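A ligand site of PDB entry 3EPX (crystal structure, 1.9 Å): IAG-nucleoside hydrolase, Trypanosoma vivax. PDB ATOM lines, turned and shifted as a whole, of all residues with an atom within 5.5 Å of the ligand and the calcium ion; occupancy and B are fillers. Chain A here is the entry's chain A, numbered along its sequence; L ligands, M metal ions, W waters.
Water W1 lies within hydrogen-bond range of the side-chain carboxylate (OD2) of Asp 21 (2.7 Å) and the side-chain amide oxygen (OD1) of Asn 197 (2.7 Å).
Of the 23 residues printed, 4 come within 4 Å of the calcium ion.
An oxygen (O2) of the ligand lies close to the side-chain amide nitrogen (ND2) of Asn 197, 3.0 Å away.
The side-chain carboxylate (OE2) of Glu 195 is in hydrogen-bond range of an oxygen (O3) of the ligand, 2.5 Å away.
The side-chain carboxylate (OD1) of Asp 25 sits close to an oxygen (O1) of the ligand, at 2.5 Å.
OD2 of Asp 51 lies within salt-bridge range of N2 of the ligand.
An oxygen (O3) of the ligand is in hydrogen-bond range of the side-chain amide nitrogen (ND2) of Asn 184, 3.1 Å away.
The calcium ion is bound by the backbone carbonyl oxygen (O) of Thr 148 (2.3 Å), the side-chain carboxylate (OD1) of Asp 21 (2.4 Å), an oxygen (O1) of the ligand (2.4 Å), the side-chain carboxylate (OD2) of Asp 272 (2.4 Å), an oxygen (O2) of the ligand (2.5 Å), the side-chain carboxylate (OD1) of Asp 26 (2.5 Å), the side-chain carboxylate (OD2) of Asp 26 (2.5 Å) and water W1 (2.6 Å).
The backbone NH (N) of Trp 196 lies within hydrogen-bond range of the side-chain amide oxygen (OD1) of Asn 184, at 2.9 Å.
O of Asp 51 is in hydrogen-bond range of ND2 of Asn 23 (3.0 Å).
The backbone carbonyl oxygen (O) of Thr 148 sits close to the side-chain amide nitrogen (ND2) of Asn 197 (3.4 Å).
The side-chain carboxylate (OD2) of Asp 26 lies close to the backbone NH (N) of Asn 23.
ND2 of Asn 197 lies within hydrogen-bond range of O of Met 175, 3.1 Å away.
N of Asp 25 lies within hydrogen-bond range of OH of Tyr 268, 3.2 Å away.
OE2 of Glu 195 lies within hydrogen-bond range of N of Asn 197.
N of Asp 272 lies within hydrogen-bond range of OD2 of Asp 25, at 2.7 Å.
Asn 23 touches the ligand (OD1 to C2, 3.7 Å).
Phe 90 touches the ligand.
CG of Trp 94 touches C3 of the ligand (3.4 Å).
Met 175 touches the ligand (SD to O2, 3.8 Å).
Trp 196 touches the ligand.
Gly 265 touches the ligand (O to C6, 3.8 Å).
CE1 of Tyr 268 touches C3 of the ligand, 3.7 Å away.
Trp 271 touches the ligand.
Hydrophobic or aromatic side chains that line the ligand: Phe 90, Trp 94, Met 175, Trp 196, Tyr 268 and Trp 271.
Along chain A the residues within 4 Å of the ligand span positions 23 to 272.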
ATOM      1  N   ASP A  21      17.166  -3.689 -20.212  1.00  0.00           N
ATOM      2  CA  ASP A  21      16.549  -4.013 -21.509  1.00  0.00           C
ATOM      3  C   ASP A  21      17.405  -4.908 -22.424  1.00  0.00           C
ATOM      4  O   ASP A  21      17.317  -4.831 -23.650  1.00  0.00           O
ATOM      5  CB  ASP A  21      16.068  -2.741 -22.243  1.00  0.00           C
ATOM      6  CG  ASP A  21      17.223  -1.858 -22.710  1.00  0.00           C
ATOM      7  OD1 ASP A  21      18.344  -1.967 -22.159  1.00  0.00           O
ATOM      8  OD2 ASP A  21      17.005  -1.065 -23.625  1.00  0.00           O
ATOM      9  N   GLY A  22      18.252  -5.746 -21.820  1.00  0.00           N
ATOM     10  CA  GLY A  22      18.757  -6.942 -22.479  1.00  0.00           C
ATOM     11  C   GLY A  22      19.752  -6.755 -23.613  1.00  0.00           C
ATOM     12  O   GLY A  22      19.884  -7.641 -24.459  1.00  0.00           O
ATOM     13  N   ASN A  23      20.440  -5.615 -23.658  1.00  0.00           N
ATOM     14  CA  ASN A  23      21.578  -5.532 -24.554  1.00  0.00           C
ATOM     15  C   ASN A  23      22.845  -6.044 -23.877  1.00  0.00           C
ATOM     16  O   ASN A  23      22.803  -6.442 -22.707  1.00  0.00           O
ATOM     17  CB  ASN A  23      21.762  -4.128 -25.135  1.00  0.00           C
ATOM     18  CG  ASN A  23      22.215  -4.178 -26.580  1.00  0.00           C
ATOM     19  OD1 ASN A  23      23.412  -4.151 -26.855  1.00  0.00           O
ATOM     20  ND2 ASN A  23      21.266  -4.345 -27.481  1.00  0.00           N
ATOM     21  N   ASP A  25      25.693  -4.769 -22.697  1.00  0.00           N
ATOM     22  CA  ASP A  25      26.148  -4.102 -21.477  1.00  0.00           C
ATOM     23  C   ASP A  25      25.165  -4.261 -20.315  1.00  0.00           C
ATOM     24  O   ASP A  25      25.586  -4.285 -19.176  1.00  0.00           O
ATOM     25  CB  ASP A  25      26.539  -2.635 -21.691  1.00  0.00           C
ATOM     26  CG  ASP A  25      25.379  -1.769 -22.044  1.00  0.00           C
ATOM     27  OD1 ASP A  25      24.396  -2.278 -22.632  1.00  0.00           O
ATOM     28  OD2 ASP A  25      25.438  -0.546 -21.722  1.00  0.00           O
ATOM     29  N   ASP A  26      23.858  -4.378 -20.615  1.00  0.00           N
ATOM     30  CA  ASP A  26      22.886  -4.716 -19.575  1.00  0.00           C
ATOM     31  C   ASP A  26      23.295  -5.986 -18.857  1.00  0.00           C
ATOM     32  O   ASP A  26      23.149  -6.087 -17.629  1.00  0.00           O
ATOM     33  CB  ASP A  26      21.472  -4.915 -20.155  1.00  0.00           C
ATOM     34  CG  ASP A  26      20.914  -3.656 -20.771  1.00  0.00           C
ATOM     35  OD1 ASP A  26      20.181  -2.901 -20.090  1.00  0.00           O
ATOM     36  OD2 ASP A  26      21.247  -3.404 -21.952  1.00  0.00           O
ATOM     37  N   ASP A  51      15.791  -2.423 -26.021  1.00  0.00           N
ATOM     38  CA  ASP A  51      17.008  -2.764 -26.780  1.00  0.00           C
ATOM     39  C   ASP A  51      17.248  -4.290 -26.819  1.00  0.00           C
ATOM     40  O   ASP A  51      18.395  -4.751 -26.864  1.00  0.00           O
ATOM     41  CB  ASP A  51      18.217  -2.027 -26.195  1.00  0.00           C
ATOM     42  CG  ASP A  51      19.294  -1.716 -27.223  1.00  0.00           C
ATOM     43  OD1 ASP A  51      19.079  -1.945 -28.424  1.00  0.00           O
ATOM     44  OD2 ASP A  51      20.374  -1.245 -26.808  1.00  0.00           O
ATOM     45  N   PHE A  90      13.673   0.788 -30.536  1.00  0.00           N
ATOM     46  CA  PHE A  90      15.081   0.675 -30.931  1.00  0.00           C
ATOM     47  C   PHE A  90      15.243   0.072 -32.338  1.00  0.00           C
ATOM     48  O   PHE A  90      14.348  -0.639 -32.815  1.00  0.00           O
ATOM     49  CB  PHE A  90      15.836  -0.206 -29.933  1.00  0.00           C
ATOM     50  CG  PHE A  90      16.315   0.528 -28.714  1.00  0.00           C
ATOM     51  CD1 PHE A  90      17.565   1.132 -28.701  1.00  0.00           C
ATOM     52  CD2 PHE A  90      15.538   0.580 -27.564  1.00  0.00           C
ATOM     53  CE1 PHE A  90      18.024   1.781 -27.580  1.00  0.00           C
ATOM     54  CE2 PHE A  90      15.992   1.260 -26.424  1.00  0.00           C
ATOM     55  CZ  PHE A  90      17.241   1.855 -26.434  1.00  0.00           C
ATOM     56  N   TRP A  94      20.104  -3.839 -33.363  1.00  0.00           N
ATOM     57  CA  TRP A  94      20.614  -3.724 -32.001  1.00  0.00           C
ATOM     58  C   TRP A  94      19.851  -4.639 -31.032  1.00  0.00           C
ATOM     59  O   TRP A  94      20.429  -5.155 -30.096  1.00  0.00           O
ATOM     60  CB  TRP A  94      20.502  -2.300 -31.484  1.00  0.00           C
ATOM     61  CG  TRP A  94      21.309  -1.271 -32.219  1.00  0.00           C
ATOM     62  CD1 TRP A  94      22.209  -1.470 -33.218  1.00  0.00           C
ATOM     63  CD2 TRP A  94      21.291   0.140 -31.968  1.00  0.00           C
ATOM     64  NE1 TRP A  94      22.757  -0.262 -33.622  1.00  0.00           N
ATOM     65  CE2 TRP A  94      22.210   0.733 -32.864  1.00  0.00           C
ATOM     66  CE3 TRP A  94      20.600   0.959 -31.064  1.00  0.00           C
ATOM     67  CZ2 TRP A  94      22.447   2.115 -32.885  1.00  0.00           C
ATOM     68  CZ3 TRP A  94      20.825   2.323 -31.090  1.00  0.00           C
ATOM     69  CH2 TRP A  94      21.740   2.897 -31.988  1.00  0.00           C
ATOM     70  N   LEU A  97      20.858  -8.733 -30.214  1.00  0.00           N
ATOM     71  CA  LEU A  97      22.073  -9.176 -29.521  1.00  0.00           C
ATOM     72  C   LEU A  97      21.792 -10.203 -28.396  1.00  0.00           C
ATOM     73  O   LEU A  97      22.600 -11.109 -28.194  1.00  0.00           O
ATOM     74  CB  LEU A  97      22.890  -7.978 -29.036  1.00  0.00           C
ATOM     75  CG  LEU A  97      23.432  -7.111 -30.188  1.00  0.00           C
ATOM     76  CD1 LEU A  97      24.168  -5.903 -29.633  1.00  0.00           C
ATOM     77  CD2 LEU A  97      24.355  -7.927 -31.094  1.00  0.00           C
ATOM     78  N   THR A 148      18.861   0.339 -16.402  1.00  0.00           N
ATOM     79  CA  THR A 148      19.811   0.298 -17.505  1.00  0.00           C
ATOM     80  C   THR A 148      19.101   0.235 -18.861  1.00  0.00           C
ATOM     81  O   THR A 148      19.740   0.180 -19.925  1.00  0.00           O
ATOM     82  CB  THR A 148      20.819  -0.869 -17.357  1.00  0.00           C
ATOM     83  OG1 THR A 148      20.107  -2.107 -17.321  1.00  0.00           O
ATOM     84  CG2 THR A 148      21.671  -0.724 -16.065  1.00  0.00           C
ATOM     85  N   GLY A 149      17.771   0.249 -18.817  1.00  0.00           N
ATOM     86  CA  GLY A 149      16.954   0.449 -20.013  1.00  0.00           C
ATOM     87  C   GLY A 149      16.079   1.672 -19.811  1.00  0.00           C
ATOM     88  O   GLY A 149      16.368   2.501 -18.934  1.00  0.00           O
ATOM     89  N   MET A 175      21.035   4.677 -16.129  1.00  0.00           N
ATOM     90  CA  MET A 175      21.803   4.963 -17.342  1.00  0.00           C
ATOM     91  C   MET A 175      20.844   5.641 -18.305  1.00  0.00           C
ATOM     92  O   MET A 175      19.850   5.047 -18.749  1.00  0.00           O
ATOM     93  CB  MET A 175      22.414   3.699 -17.965  1.00  0.00           C
ATOM     94  CG  MET A 175      23.470   3.985 -19.049  1.00  0.00           C
ATOM     95  SD  MET A 175      22.727   4.522 -20.593  1.00  0.00           S
ATOM     96  CE  MET A 175      23.711   6.004 -20.947  1.00  0.00           C
ATOM     97  N   ASN A 184      22.780  10.302 -28.691  1.00  0.00           N
ATOM     98  CA  ASN A 184      23.142   9.231 -29.600  1.00  0.00           C
ATOM     99  C   ASN A 184      21.991   8.760 -30.483  1.00  0.00           C
ATOM    100  O   ASN A 184      22.077   7.700 -31.108  1.00  0.00           O
ATOM    101  CB  ASN A 184      23.821   8.068 -28.834  1.00  0.00           C
ATOM    102  CG  ASN A 184      22.901   7.429 -27.801  1.00  0.00           C
ATOM    103  OD1 ASN A 184      21.689   7.639 -27.803  1.00  0.00           O
ATOM    104  ND2 ASN A 184      23.482   6.611 -26.930  1.00  0.00           N
ATOM    105  N   GLU A 195      19.396  10.860 -25.996  1.00  0.00           N
ATOM    106  CA  GLU A 195      19.991   9.551 -25.766  1.00  0.00           C
ATOM    107  C   GLU A 195      18.877   8.512 -25.814  1.00  0.00           C
ATOM    108  O   GLU A 195      17.719   8.800 -25.463  1.00  0.00           O
ATOM    109  CB  GLU A 195      20.725   9.540 -24.416  1.00  0.00           C
ATOM    110  CG  GLU A 195      21.377   8.215 -24.020  1.00  0.00           C
ATOM    111  CD  GLU A 195      20.358   7.235 -23.432  1.00  0.00           C
ATOM    112  OE1 GLU A 195      19.385   7.695 -22.810  1.00  0.00           O
ATOM    113  OE2 GLU A 195      20.531   6.010 -23.609  1.00  0.00           O
ATOM    114  N   TRP A 196      19.225   7.301 -26.250  1.00  0.00           N
ATOM    115  CA  TRP A 196      18.253   6.285 -26.643  1.00  0.00           C
ATOM    116  C   TRP A 196      17.319   5.796 -25.532  1.00  0.00           C
ATOM    117  O   TRP A 196      16.122   5.640 -25.773  1.00  0.00           O
ATOM    118  CB  TRP A 196      18.956   5.110 -27.345  1.00  0.00           C
ATOM    119  CG  TRP A 196      18.896   5.215 -28.851  1.00  0.00           C
ATOM    120  CD1 TRP A 196      19.908   5.569 -29.701  1.00  0.00           C
ATOM    121  CD2 TRP A 196      17.751   4.994 -29.661  1.00  0.00           C
ATOM    122  NE1 TRP A 196      19.457   5.544 -31.012  1.00  0.00           N
ATOM    123  CE2 TRP A 196      18.130   5.205 -31.008  1.00  0.00           C
ATOM    124  CE3 TRP A 196      16.423   4.623 -29.385  1.00  0.00           C
ATOM    125  CZ2 TRP A 196      17.230   5.068 -32.077  1.00  0.00           C
ATOM    126  CZ3 TRP A 196      15.526   4.475 -30.463  1.00  0.00           C
ATOM    127  CH2 TRP A 196      15.939   4.700 -31.782  1.00  0.00           C
ATOM    128  N   ASN A 197      17.846   5.541 -24.350  1.00  0.00           N
ATOM    129  CA  ASN A 197      16.988   5.041 -23.256  1.00  0.00           C
ATOM    130  C   ASN A 197      15.845   5.996 -22.923  1.00  0.00           C
ATOM    131  O   ASN A 197      14.723   5.574 -22.684  1.00  0.00           O
ATOM    132  CB  ASN A 197      17.804   4.728 -22.010  1.00  0.00           C
ATOM    133  CG  ASN A 197      18.669   3.505 -22.172  1.00  0.00           C
ATOM    134  OD1 ASN A 197      18.536   2.757 -23.140  1.00  0.00           O
ATOM    135  ND2 ASN A 197      19.569   3.282 -21.225  1.00  0.00           N
ATOM    136  N   LEU A 221      25.506  10.297 -21.077  1.00  0.00           N
ATOM    137  CA  LEU A 221      26.616  10.143 -22.024  1.00  0.00           C
ATOM    138  C   LEU A 221      27.856  10.966 -21.640  1.00  0.00           C
ATOM    139  O   LEU A 221      28.983  10.623 -22.017  1.00  0.00           O
ATOM    140  CB  LEU A 221      26.151  10.480 -23.448  1.00  0.00           C
ATOM    141  CG  LEU A 221      25.013   9.641 -24.048  1.00  0.00           C
ATOM    142  CD1 LEU A 221      24.916   9.883 -25.546  1.00  0.00           C
ATOM    143  CD2 LEU A 221      25.235   8.156 -23.782  1.00  0.00           C
ATOM    144  N   GLY A 265      27.651   7.499 -34.065  1.00  0.00           N
ATOM    145  CA  GLY A 265      26.567   7.183 -33.131  1.00  0.00           C
ATOM    146  C   GLY A 265      26.355   5.706 -32.867  1.00  0.00           C
ATOM    147  O   GLY A 265      25.631   5.344 -31.934  1.00  0.00           O
ATOM    148  N   ASP A 266      26.982   4.862 -33.680  1.00  0.00           N
ATOM    149  CA  ASP A 266      26.850   3.417 -33.511  1.00  0.00           C
ATOM    150  C   ASP A 266      27.884   2.838 -32.546  1.00  0.00           C
ATOM    151  O   ASP A 266      27.798   1.652 -32.205  1.00  0.00           O
ATOM    152  CB  ASP A 266      26.956   2.699 -34.874  1.00  0.00           C
ATOM    153  CG  ASP A 266      25.712   2.880 -35.730  1.00  0.00           C
ATOM    154  OD1 ASP A 266      24.821   3.683 -35.360  1.00  0.00           O
ATOM    155  OD2 ASP A 266      25.616   2.211 -36.783  1.00  0.00           O
ATOM    156  N   GLY A 267      28.838   3.662 -32.099  1.00  0.00           N
ATOM    157  CA  GLY A 267      29.936   3.228 -31.208  1.00  0.00           C
ATOM    158  C   GLY A 267      29.431   2.644 -29.901  1.00  0.00           C
ATOM    159  O   GLY A 267      28.469   3.135 -29.331  1.00  0.00           O
ATOM    160  N   TYR A 268      30.076   1.570 -29.428  1.00  0.00           N
ATOM    161  CA  TYR A 268      29.621   0.890 -28.204  1.00  0.00           C
ATOM    162  C   TYR A 268      30.480   1.301 -27.010  1.00  0.00           C
ATOM    163  O   TYR A 268      31.704   1.408 -27.138  1.00  0.00           O
ATOM    164  CB  TYR A 268      29.646  -0.637 -28.379  1.00  0.00           C
ATOM    165  CG  TYR A 268      28.548  -1.378 -27.627  1.00  0.00           C
ATOM    166  CD1 TYR A 268      27.381  -1.775 -28.284  1.00  0.00           C
ATOM    167  CD2 TYR A 268      28.674  -1.689 -26.270  1.00  0.00           C
ATOM    168  CE1 TYR A 268      26.361  -2.465 -27.595  1.00  0.00           C
ATOM    169  CE2 TYR A 268      27.674  -2.363 -25.572  1.00  0.00           C
ATOM    170  CZ  TYR A 268      26.518  -2.750 -26.245  1.00  0.00           C
ATOM    171  OH  TYR A 268      25.523  -3.424 -25.555  1.00  0.00           O
ATOM    172  N   TRP A 271      28.181   1.622 -21.119  1.00  0.00           N
ATOM    173  CA  TRP A 271      27.187   2.522 -20.525  1.00  0.00           C
ATOM    174  C   TRP A 271      26.586   1.924 -19.258  1.00  0.00           C
ATOM    175  O   TRP A 271      26.661   2.515 -18.190  1.00  0.00           O
ATOM    176  CB  TRP A 271      26.003   2.779 -21.466  1.00  0.00           C
ATOM    177  CG  TRP A 271      26.252   3.337 -22.861  1.00  0.00           C
ATOM    178  CD1 TRP A 271      26.400   4.656 -23.209  1.00  0.00           C
ATOM    179  CD2 TRP A 271      26.257   2.598 -24.085  1.00  0.00           C
ATOM    180  NE1 TRP A 271      26.532   4.765 -24.580  1.00  0.00           N
ATOM    181  CE2 TRP A 271      26.447   3.516 -25.141  1.00  0.00           C
ATOM    182  CE3 TRP A 271      26.129   1.233 -24.392  1.00  0.00           C
ATOM    183  CZ2 TRP A 271      26.497   3.110 -26.490  1.00  0.00           C
ATOM    184  CZ3 TRP A 271      26.177   0.838 -25.731  1.00  0.00           C
ATOM    185  CH2 TRP A 271      26.378   1.772 -26.759  1.00  0.00           C
ATOM    186  N   ASP A 272      25.964   0.751 -19.392  1.00  0.00           N
ATOM    187  CA  ASP A 272      25.243   0.147 -18.266  1.00  0.00           C
ATOM    188  C   ASP A 272      26.185  -0.430 -17.237  1.00  0.00           C
ATOM    189  O   ASP A 272      25.850  -0.499 -16.054  1.00  0.00           O
ATOM    190  CB  ASP A 272      24.273  -0.926 -18.746  1.00  0.00           C
ATOM    191  CG  ASP A 272      23.219  -0.385 -19.708  1.00  0.00           C
ATOM    192  OD1 ASP A 272      23.045   0.851 -19.781  1.00  0.00           O
ATOM    193  OD2 ASP A 272      22.558  -1.195 -20.375  1.00  0.00           O
HETATM  194  C1  LIG L   1      22.883   0.968 -28.525  1.00  0.00           C
HETATM  195  N1  LIG L   1      22.423  -0.294 -28.367  1.00  0.00           N
HETATM  196  C2  LIG L   1      22.889  -1.309 -29.088  1.00  0.00           C
HETATM  197  C3  LIG L   1      23.881  -1.119 -30.042  1.00  0.00           C
HETATM  198  C4  LIG L   1      24.392   0.167 -30.243  1.00  0.00           C
HETATM  199  C5  LIG L   1      23.894   1.215 -29.473  1.00  0.00           C
HETATM  200  C6  LIG L   1      24.395   2.502 -29.656  1.00  0.00           C
HETATM  201  C7  LIG L   1      23.886   3.542 -28.891  1.00  0.00           C
HETATM  202  C8  LIG L   1      22.886   3.303 -27.938  1.00  0.00           C
HETATM  203  C9  LIG L   1      22.375   2.016 -27.715  1.00  0.00           C
HETATM  204  C10 LIG L   1      21.253   1.913 -26.640  1.00  0.00           C
HETATM  205  N2  LIG L   1      21.672   1.424 -25.268  1.00  0.00           N
HETATM  206  C11 LIG L   1      22.776   0.470 -25.270  1.00  0.00           C
HETATM  207  C12 LIG L   1      23.050   0.282 -23.783  1.00  0.00           C
HETATM  208  O1  LIG L   1      22.360  -0.897 -23.297  1.00  0.00           O
HETATM  209  C13 LIG L   1      22.519   1.551 -23.073  1.00  0.00           C
HETATM  210  O2  LIG L   1      21.582   1.177 -22.025  1.00  0.00           O
HETATM  211  C14 LIG L   1      21.829   2.395 -24.161  1.00  0.00           C
HETATM  212  C15 LIG L   1      22.732   3.595 -24.501  1.00  0.00           C
HETATM  213  O3  LIG L   1      21.999   4.629 -25.144  1.00  0.00           O
HETATM  214 CA    CA M   1      20.511  -1.029 -21.710  1.00  0.00          CA
HETATM  215  O   HOH W   1      19.333   0.230 -23.614  1.00  0.00           O
